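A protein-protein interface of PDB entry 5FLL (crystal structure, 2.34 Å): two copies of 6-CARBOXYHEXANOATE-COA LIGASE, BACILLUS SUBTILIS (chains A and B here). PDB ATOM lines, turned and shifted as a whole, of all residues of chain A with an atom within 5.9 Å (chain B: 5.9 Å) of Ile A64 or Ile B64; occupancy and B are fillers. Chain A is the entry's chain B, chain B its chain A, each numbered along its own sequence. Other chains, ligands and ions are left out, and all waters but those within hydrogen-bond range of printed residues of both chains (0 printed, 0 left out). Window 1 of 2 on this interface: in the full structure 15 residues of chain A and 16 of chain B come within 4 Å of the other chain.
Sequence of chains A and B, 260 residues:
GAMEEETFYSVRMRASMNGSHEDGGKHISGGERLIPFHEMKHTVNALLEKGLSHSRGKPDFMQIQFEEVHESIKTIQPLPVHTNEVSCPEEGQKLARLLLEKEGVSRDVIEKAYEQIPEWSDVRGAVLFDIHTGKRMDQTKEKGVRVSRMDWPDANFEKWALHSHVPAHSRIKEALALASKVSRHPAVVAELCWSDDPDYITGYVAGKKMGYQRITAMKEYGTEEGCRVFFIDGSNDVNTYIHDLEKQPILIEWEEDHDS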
ATOM      1  N   VAL A  11     -16.271  26.325 -15.844  1.00  0.00           N
ATOM      2  CA  VAL A  11     -15.111  25.546 -15.399  1.00  0.00           C
ATOM      3  C   VAL A  11     -13.902  26.441 -15.473  1.00  0.00           C
ATOM      4  O   VAL A  11     -13.619  27.030 -16.521  1.00  0.00           O
ATOM      5  CB  VAL A  11     -14.905  24.282 -16.238  1.00  0.00           C
ATOM      6  CG1 VAL A  11     -13.901  23.374 -15.564  1.00  0.00           C
ATOM      7  CG2 VAL A  11     -16.236  23.568 -16.393  1.00  0.00           C
ATOM      8  N   ARG A  12     -13.218  26.561 -14.353  1.00  0.00           N
ATOM      9  CA  ARG A  12     -12.090  27.466 -14.244  1.00  0.00           C
ATOM     10  C   ARG A  12     -10.868  26.762 -13.668  1.00  0.00           C
ATOM     11  O   ARG A  12     -10.979  25.850 -12.861  1.00  0.00           O
ATOM     12  CB  ARG A  12     -12.457  28.614 -13.360  1.00  0.00           C
ATOM     13  CG  ARG A  12     -13.578  29.445 -13.923  1.00  0.00           C
ATOM     14  CD  ARG A  12     -13.923  30.617 -13.012  1.00  0.00           C
ATOM     15  NE  ARG A  12     -14.735  30.166 -11.898  1.00  0.00           N
ATOM     16  CZ  ARG A  12     -14.922  30.840 -10.779  1.00  0.00           C
ATOM     17  NH1 ARG A  12     -14.358  32.015 -10.616  1.00  0.00           N
ATOM     18  NH2 ARG A  12     -15.675  30.325  -9.835  1.00  0.00           N
ATOM     19  N   MET A  13      -9.700  27.248 -14.061  1.00  0.00           N
ATOM     20  CA  MET A  13      -8.425  26.739 -13.578  1.00  0.00           C
ATOM     21  C   MET A  13      -7.456  27.902 -13.318  1.00  0.00           C
ATOM     22  O   MET A  13      -7.470  28.904 -14.024  1.00  0.00           O
ATOM     23  CB  MET A  13      -7.822  25.803 -14.632  1.00  0.00           C
ATOM     24  CG  MET A  13      -6.455  25.247 -14.280  1.00  0.00           C
ATOM     25  SD  MET A  13      -5.098  26.303 -14.810  1.00  0.00           S
ATOM     26  CE  MET A  13      -5.185  26.180 -16.590  1.00  0.00           C
ATOM     27  N   ARG A  14      -6.613  27.764 -12.314  1.00  0.00           N
ATOM     28  CA  ARG A  14      -5.448  28.610 -12.247  1.00  0.00           C
ATOM     29  C   ARG A  14      -4.279  27.826 -11.674  1.00  0.00           C
ATOM     30  O   ARG A  14      -4.457  26.922 -10.838  1.00  0.00           O
ATOM     31  CB  ARG A  14      -5.726  29.868 -11.430  1.00  0.00           C
ATOM     32  CG  ARG A  14      -6.311  29.571 -10.090  1.00  0.00           C
ATOM     33  CD  ARG A  14      -6.585  30.847  -9.291  1.00  0.00           C
ATOM     34  NE  ARG A  14      -7.166  30.487  -8.010  1.00  0.00           N
ATOM     35  CZ  ARG A  14      -6.505  30.470  -6.852  1.00  0.00           C
ATOM     36  NH1 ARG A  14      -5.228  30.841  -6.801  1.00  0.00           N
ATOM     37  NH2 ARG A  14      -7.131  30.089  -5.744  1.00  0.00           N
ATOM     38  N   VAL A  44     -12.161  19.270 -17.905  1.00  0.00           N
ATOM     39  CA  VAL A  44     -11.282  19.270 -16.719  1.00  0.00           C
ATOM     40  C   VAL A  44      -9.870  18.804 -17.084  1.00  0.00           C
ATOM     41  O   VAL A  44      -8.873  19.410 -16.680  1.00  0.00           O
ATOM     42  CB  VAL A  44     -11.861  18.431 -15.559  1.00  0.00           C
ATOM     43  CG1 VAL A  44     -10.787  18.129 -14.515  1.00  0.00           C
ATOM     44  CG2 VAL A  44     -13.025  19.182 -14.902  1.00  0.00           C
ATOM     45  N   LEU A  47      -8.059  21.585 -19.165  1.00  0.00           N
ATOM     46  CA  LEU A  47      -7.524  22.622 -18.312  1.00  0.00           C
ATOM     47  C   LEU A  47      -6.318  22.102 -17.518  1.00  0.00           C
ATOM     48  O   LEU A  47      -5.325  22.822 -17.317  1.00  0.00           O
ATOM     49  CB  LEU A  47      -8.604  23.125 -17.384  1.00  0.00           C
ATOM     50  CG  LEU A  47      -9.707  23.966 -18.054  1.00  0.00           C
ATOM     51  CD1 LEU A  47     -10.930  24.111 -17.142  1.00  0.00           C
ATOM     52  CD2 LEU A  47      -9.189  25.357 -18.422  1.00  0.00           C
ATOM     53  N   LEU A  48      -6.411  20.867 -17.038  1.00  0.00           N
ATOM     54  CA  LEU A  48      -5.301  20.276 -16.292  1.00  0.00           C
ATOM     55  C   LEU A  48      -4.055  20.268 -17.184  1.00  0.00           C
ATOM     56  O   LEU A  48      -3.006  20.757 -16.804  1.00  0.00           O
ATOM     57  CB  LEU A  48      -5.658  18.856 -15.876  1.00  0.00           C
ATOM     58  CG  LEU A  48      -4.572  18.102 -15.112  1.00  0.00           C
ATOM     59  CD1 LEU A  48      -4.186  18.814 -13.808  1.00  0.00           C
ATOM     60  CD2 LEU A  48      -5.054  16.686 -14.843  1.00  0.00           C
ATOM     61  N   MET A  62      -2.311  24.226  -8.258  1.00  0.00           N
ATOM     62  CA  MET A  62      -3.335  24.374  -9.246  1.00  0.00           C
ATOM     63  C   MET A  62      -4.701  24.192  -8.624  1.00  0.00           C
ATOM     64  O   MET A  62      -4.895  23.360  -7.744  1.00  0.00           O
ATOM     65  CB  MET A  62      -3.138  23.376 -10.393  1.00  0.00           C
ATOM     66  CG  MET A  62      -4.244  23.414 -11.451  1.00  0.00           C
ATOM     67  SD  MET A  62      -3.962  22.350 -12.921  1.00  0.00           S
ATOM     68  CE  MET A  62      -2.217  22.598 -13.188  1.00  0.00           C
ATOM     69  N   GLN A  63      -5.644  24.984  -9.092  1.00  0.00           N
ATOM     70  CA  GLN A  63      -7.013  24.831  -8.691  1.00  0.00           C
ATOM     71  C   GLN A  63      -7.907  24.694  -9.899  1.00  0.00           C
ATOM     72  O   GLN A  63      -7.802  25.464 -10.843  1.00  0.00           O
ATOM     73  CB  GLN A  63      -7.437  26.016  -7.870  1.00  0.00           C
ATOM     74  CG  GLN A  63      -8.642  25.697  -7.038  1.00  0.00           C
ATOM     75  CD  GLN A  63      -9.117  26.886  -6.230  1.00  0.00           C
ATOM     76  OE1 GLN A  63      -8.344  27.489  -5.461  1.00  0.00           O
ATOM     77  NE2 GLN A  63     -10.398  27.217  -6.377  1.00  0.00           N
ATOM     78  N   ILE A  64      -8.798  23.716  -9.871  1.00  0.00           N
ATOM     79  CA  ILE A  64      -9.801  23.560 -10.933  1.00  0.00           C
ATOM     80  C   ILE A  64     -11.160  23.486 -10.289  1.00  0.00           C
ATOM     81  O   ILE A  64     -11.344  22.837  -9.256  1.00  0.00           O
ATOM     82  CB  ILE A  64      -9.616  22.285 -11.747  1.00  0.00           C
ATOM     83  CG1 ILE A  64      -8.251  22.268 -12.409  1.00  0.00           C
ATOM     84  CG2 ILE A  64     -10.701  22.175 -12.822  1.00  0.00           C
ATOM     85  CD1 ILE A  64      -7.972  21.038 -13.265  1.00  0.00           C
ATOM     86  N   GLN A  65     -12.133  24.139 -10.899  1.00  0.00           N
ATOM     87  CA  GLN A  65     -13.385  24.362 -10.217  1.00  0.00           C
ATOM     88  C   GLN A  65     -14.513  24.344 -11.221  1.00  0.00           C
ATOM     89  O   GLN A  65     -14.368  24.868 -12.325  1.00  0.00           O
ATOM     90  CB  GLN A  65     -13.313  25.712  -9.552  1.00  0.00           C
ATOM     91  CG  GLN A  65     -14.344  25.921  -8.479  1.00  0.00           C
ATOM     92  CD  GLN A  65     -14.277  27.325  -7.964  1.00  0.00           C
ATOM     93  OE1 GLN A  65     -13.216  27.944  -8.036  1.00  0.00           O
ATOM     94  NE2 GLN A  65     -15.415  27.873  -7.531  1.00  0.00           N
ATOM     95  N   PHE A  66     -15.638  23.727 -10.877  1.00  0.00           N
ATOM     96  CA  PHE A  66     -16.831  23.952 -11.675  1.00  0.00           C
ATOM     97  C   PHE A  66     -18.026  24.340 -10.830  1.00  0.00           C
ATOM     98  O   PHE A  66     -18.077  24.025  -9.649  1.00  0.00           O
ATOM     99  CB  PHE A  66     -17.135  22.814 -12.665  1.00  0.00           C
ATOM    100  CG  PHE A  66     -17.715  21.591 -12.054  1.00  0.00           C
ATOM    101  CD1 PHE A  66     -19.013  21.578 -11.590  1.00  0.00           C
ATOM    102  CD2 PHE A  66     -16.993  20.410 -12.046  1.00  0.00           C
ATOM    103  CE1 PHE A  66     -19.577  20.418 -11.071  1.00  0.00           C
ATOM    104  CE2 PHE A  66     -17.537  19.238 -11.522  1.00  0.00           C
ATOM    105  CZ  PHE A  66     -18.836  19.240 -11.028  1.00  0.00           C
ATOM    106  N   VAL B  11      -3.469  16.494  -2.964  1.00  0.00           N
ATOM    107  CA  VAL B  11      -4.535  16.667  -3.954  1.00  0.00           C
ATOM    108  C   VAL B  11      -5.850  16.431  -3.235  1.00  0.00           C
ATOM    109  O   VAL B  11      -6.067  15.369  -2.598  1.00  0.00           O
ATOM    110  CB  VAL B  11      -4.415  15.710  -5.152  1.00  0.00           C
ATOM    111  CG1 VAL B  11      -5.290  16.180  -6.300  1.00  0.00           C
ATOM    112  CG2 VAL B  11      -2.973  15.600  -5.626  1.00  0.00           C
ATOM    113  N   ARG B  12      -6.690  17.467  -3.292  1.00  0.00           N
ATOM    114  CA  ARG B  12      -7.943  17.518  -2.557  1.00  0.00           C
ATOM    115  C   ARG B  12      -9.108  17.847  -3.470  1.00  0.00           C
ATOM    116  O   ARG B  12      -8.956  18.575  -4.458  1.00  0.00           O
ATOM    117  CB  ARG B  12      -7.872  18.579  -1.459  1.00  0.00           C
ATOM    118  CG  ARG B  12      -6.848  18.237  -0.397  1.00  0.00           C
ATOM    119  CD  ARG B  12      -6.936  19.207   0.764  1.00  0.00           C
ATOM    120  NE  ARG B  12      -6.274  20.448   0.456  1.00  0.00           N
ATOM    121  CZ  ARG B  12      -6.512  21.605   1.054  1.00  0.00           C
ATOM    122  NH1 ARG B  12      -7.489  21.725   1.960  1.00  0.00           N
ATOM    123  NH2 ARG B  12      -5.755  22.648   0.737  1.00  0.00           N
ATOM    124  N   MET B  13     -10.278  17.382  -3.051  1.00  0.00           N
ATOM    125  CA  MET B  13     -11.496  17.607  -3.771  1.00  0.00           C
ATOM    126  C   MET B  13     -12.621  17.825  -2.764  1.00  0.00           C
ATOM    127  O   MET B  13     -12.668  17.187  -1.708  1.00  0.00           O
ATOM    128  CB  MET B  13     -11.810  16.377  -4.649  1.00  0.00           C
ATOM    129  CG  MET B  13     -13.124  16.448  -5.422  1.00  0.00           C
ATOM    130  SD  MET B  13     -14.523  15.838  -4.476  1.00  0.00           S
ATOM    131  CE  MET B  13     -14.199  14.087  -4.408  1.00  0.00           C
ATOM    132  N   ARG B  14     -13.572  18.676  -3.121  1.00  0.00           N
ATOM    133  CA  ARG B  14     -14.855  18.642  -2.456  1.00  0.00           C
ATOM    134  C   ARG B  14     -15.958  18.972  -3.458  1.00  0.00           C
ATOM    135  O   ARG B  14     -15.742  19.727  -4.431  1.00  0.00           O
ATOM    136  CB  ARG B  14     -14.897  19.604  -1.280  1.00  0.00           C
ATOM    137  CG  ARG B  14     -14.448  20.969  -1.677  1.00  0.00           C
ATOM    138  CD  ARG B  14     -14.530  21.974  -0.553  1.00  0.00           C
ATOM    139  NE  ARG B  14     -14.187  23.282  -1.082  1.00  0.00           N
ATOM    140  CZ  ARG B  14     -14.391  24.412  -0.437  1.00  0.00           C
ATOM    141  NH1 ARG B  14     -14.963  24.391   0.761  1.00  0.00           N
ATOM    142  NH2 ARG B  14     -14.039  25.562  -0.991  1.00  0.00           N
ATOM    143  N   VAL B  44      -6.252  13.239 -10.221  1.00  0.00           N
ATOM    144  CA  VAL B  44      -7.266  14.262 -10.457  1.00  0.00           C
ATOM    145  C   VAL B  44      -8.522  13.624 -11.042  1.00  0.00           C
ATOM    146  O   VAL B  44      -9.631  13.926 -10.595  1.00  0.00           O
ATOM    147  CB  VAL B  44      -6.743  15.380 -11.385  1.00  0.00           C
ATOM    148  CG1 VAL B  44      -7.889  16.214 -11.928  1.00  0.00           C
ATOM    149  CG2 VAL B  44      -5.768  16.277 -10.622  1.00  0.00           C
ATOM    150  N   LEU B  47     -10.435  11.553  -8.334  1.00  0.00           N
ATOM    151  CA  LEU B  47     -11.208  12.442  -7.457  1.00  0.00           C
ATOM    152  C   LEU B  47     -12.408  13.035  -8.177  1.00  0.00           C
ATOM    153  O   LEU B  47     -13.513  13.110  -7.628  1.00  0.00           O
ATOM    154  CB  LEU B  47     -10.320  13.553  -6.917  1.00  0.00           C
ATOM    155  CG  LEU B  47      -9.271  13.140  -5.888  1.00  0.00           C
ATOM    156  CD1 LEU B  47      -8.218  14.216  -5.708  1.00  0.00           C
ATOM    157  CD2 LEU B  47      -9.897  12.830  -4.533  1.00  0.00           C
ATOM    158  N   LEU B  48     -12.202  13.413  -9.433  1.00  0.00           N
ATOM    159  CA  LEU B  48     -13.298  13.867 -10.259  1.00  0.00           C
ATOM    160  C   LEU B  48     -14.395  12.796 -10.305  1.00  0.00           C
ATOM    161  O   LEU B  48     -15.565  13.076 -10.029  1.00  0.00           O
ATOM    162  CB  LEU B  48     -12.798  14.184 -11.659  1.00  0.00           C
ATOM    163  CG  LEU B  48     -13.848  14.712 -12.635  1.00  0.00           C
ATOM    164  CD1 LEU B  48     -14.511  16.010 -12.137  1.00  0.00           C
ATOM    165  CD2 LEU B  48     -13.213  14.914 -13.993  1.00  0.00           C
ATOM    166  N   MET B  62     -17.880  21.747  -7.657  1.00  0.00           N
ATOM    167  CA  MET B  62     -16.722  20.943  -7.248  1.00  0.00           C
ATOM    168  C   MET B  62     -15.430  21.734  -7.366  1.00  0.00           C
ATOM    169  O   MET B  62     -15.285  22.566  -8.237  1.00  0.00           O
ATOM    170  CB  MET B  62     -16.630  19.672  -8.088  1.00  0.00           C
ATOM    171  CG  MET B  62     -15.410  18.791  -7.791  1.00  0.00           C
ATOM    172  SD  MET B  62     -15.306  17.216  -8.712  1.00  0.00           S
ATOM    173  CE  MET B  62     -17.049  16.724  -8.736  1.00  0.00           C
ATOM    174  N   GLN B  63     -14.501  21.458  -6.459  1.00  0.00           N
ATOM    175  CA  GLN B  63     -13.180  22.042  -6.468  1.00  0.00           C
ATOM    176  C   GLN B  63     -12.164  20.936  -6.343  1.00  0.00           C
ATOM    177  O   GLN B  63     -12.258  20.069  -5.460  1.00  0.00           O
ATOM    178  CB  GLN B  63     -12.972  22.962  -5.267  1.00  0.00           C
ATOM    179  CG  GLN B  63     -13.413  24.380  -5.491  1.00  0.00           C
ATOM    180  CD  GLN B  63     -13.297  25.294  -4.268  1.00  0.00           C
ATOM    181  OE1 GLN B  63     -13.230  24.846  -3.111  1.00  0.00           O
ATOM    182  NE2 GLN B  63     -13.301  26.598  -4.530  1.00  0.00           N
ATOM    183  N   ILE B  64     -11.141  20.997  -7.164  1.00  0.00           N
ATOM    184  CA  ILE B  64     -10.027  20.081  -7.041  1.00  0.00           C
ATOM    185  C   ILE B  64      -8.786  20.928  -7.016  1.00  0.00           C
ATOM    186  O   ILE B  64      -8.649  21.871  -7.787  1.00  0.00           O
ATOM    187  CB  ILE B  64      -9.923  19.147  -8.253  1.00  0.00           C
ATOM    188  CG1 ILE B  64     -11.199  18.308  -8.369  1.00  0.00           C
ATOM    189  CG2 ILE B  64      -8.714  18.255  -8.125  1.00  0.00           C
ATOM    190  CD1 ILE B  64     -11.219  17.317  -9.544  1.00  0.00           C
ATOM    191  N   GLN B  65      -7.842  20.547  -6.188  1.00  0.00           N
ATOM    192  CA  GLN B  65      -6.728  21.411  -5.910  1.00  0.00           C
ATOM    193  C   GLN B  65      -5.495  20.564  -5.662  1.00  0.00           C
ATOM    194  O   GLN B  65      -5.585  19.552  -4.986  1.00  0.00           O
ATOM    195  CB  GLN B  65      -7.040  22.224  -4.659  1.00  0.00           C
ATOM    196  CG  GLN B  65      -6.165  23.444  -4.522  1.00  0.00           C
ATOM    197  CD  GLN B  65      -6.343  24.173  -3.202  1.00  0.00           C
ATOM    198  OE1 GLN B  65      -7.217  25.023  -3.070  1.00  0.00           O
ATOM    199  NE2 GLN B  65      -5.462  23.880  -2.242  1.00  0.00           N
ATOM    200  N   PHE B  66      -4.337  20.977  -6.189  1.00  0.00           N
ATOM    201  CA  PHE B  66      -3.084  20.391  -5.719  1.00  0.00           C
ATOM    202  C   PHE B  66      -2.071  21.430  -5.298  1.00  0.00           C
ATOM    203  O   PHE B  66      -2.127  22.572  -5.731  1.00  0.00           O
ATOM    204  CB  PHE B  66      -2.501  19.361  -6.694  1.00  0.00           C
ATOM    205  CG  PHE B  66      -1.846  19.935  -7.914  1.00  0.00           C
ATOM    206  CD1 PHE B  66      -0.615  20.540  -7.831  1.00  0.00           C
ATOM    207  CD2 PHE B  66      -2.423  19.756  -9.176  1.00  0.00           C
ATOM    208  CE1 PHE B  66       0.023  21.027  -8.971  1.00  0.00           C
ATOM    209  CE2 PHE B  66      -1.785  20.208 -10.328  1.00  0.00           C
ATOM    210  CZ  PHE B  66      -0.567  20.868 -10.221  1.00  0.00           C
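Of the 12 printed residues of chain A, 5 touch a printed residue of chain B.
Printed residues of chain A that touch a printed residue of chain B: Met A62, Gln A63, Ile A64, Gln A65 and Phe A66.
Hydrophobic or aromatic side chains of chain A that line the printed part of chain B: Met A62 and Phe A66.
Printed residues of chain B that touch a printed residue of chain A: Met B62, Gln B63, Ile B64, Gln B65 and Phe B66.
Hydrophobic or aromatic side chains of chain B that line the printed part of chain A: Met B62 and Phe B66.
Among the printed residues, 10 pairs touch across the chains.
Ile A64 touches just these residues of chain B: Gln B63 (3.4 Å) and Ile B64 (2.8 Å).
Ile B64 touches just these residues of chain A: Gln A63 and Ile A64.
Of the printed residues of chain A, Met B62 touches Gln A65 and Phe A66.
Printed residues of chain A within 4 Å of Gln B65: Met A62 (3.2 Å) and Gln A63 (3.6 Å).
Met B13 touches none of the printed residues of chain A.
Val A44 touches none of the printed residues of chain B.
The nearest printed residue of chain B that does not touch Met A62 is Ile B64 (4.04 Å).
N of Gln B65 sits at hydrogen-bond distance from O of Arg B12, 2.9 Å away.
The side-chain amide oxygen (OE1) of Gln B63 sits at hydrogen-bond distance from the guanidinium group (NE) of Arg B14.
O of Arg A12 lies within hydrogen-bond range of N of Gln A65, 2.8 Å away.
The backbone carbonyl oxygen (O) of Arg A14 sits at hydrogen-bond distance from the backbone NH (N) of Gln A63, at 2.9 Å.
The side-chain amide oxygen of Gln A65 sits at hydrogen-bond distance from the side-chain amide nitrogen of Gln A63 (3.3 Å).
Met A62 touches Gln B65, and with the chains exchanged Gln A65 touches Met B62.
Met A62 touches Phe B66, and with the chains exchanged Phe A66 touches Met B62.
Gln A63 touches its own counterpart, Gln B63.
Gln A63 touches Gln B65, and with the chains exchanged Gln A65 touches Gln B63.
Positions printed for both chains: 11, 12, 13, 14, 44, 47, 48, 62, 63, 64, 65 and 66.
Of the 10 pairs that touch across the chains among the printed residues, 10 have their exchanged pair printed and touching as well.
Met A62 touches Gln B65 (O to CA, 3.2 Å).
Ile B64 touches Gln A63.
Gln B65 touches Gln A63 (OE1 to OE1, 3.6 Å).
Ile A64 touches Gln B63 (O to CA, 3.4 Å).
Met B62 touches Gln A65.
CG of Gln B63 touches CG of Gln A65 (3.5 Å).
N of Phe A66 lies within hydrogen-bond range of O of Met B62, at 2.9 Å.
NE2 of Gln B63 sits close to NE2 of Gln A63 (3.5 Å).
The backbone carbonyl oxygen (O) of Ile B64 lies within hydrogen-bond range of the backbone NH (N) of Ile A64 (2.8 Å).
The backbone carbonyl oxygen (O) of Met A62 is in hydrogen-bond range of the backbone NH (N) of Phe B66, at 2.9 Å.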
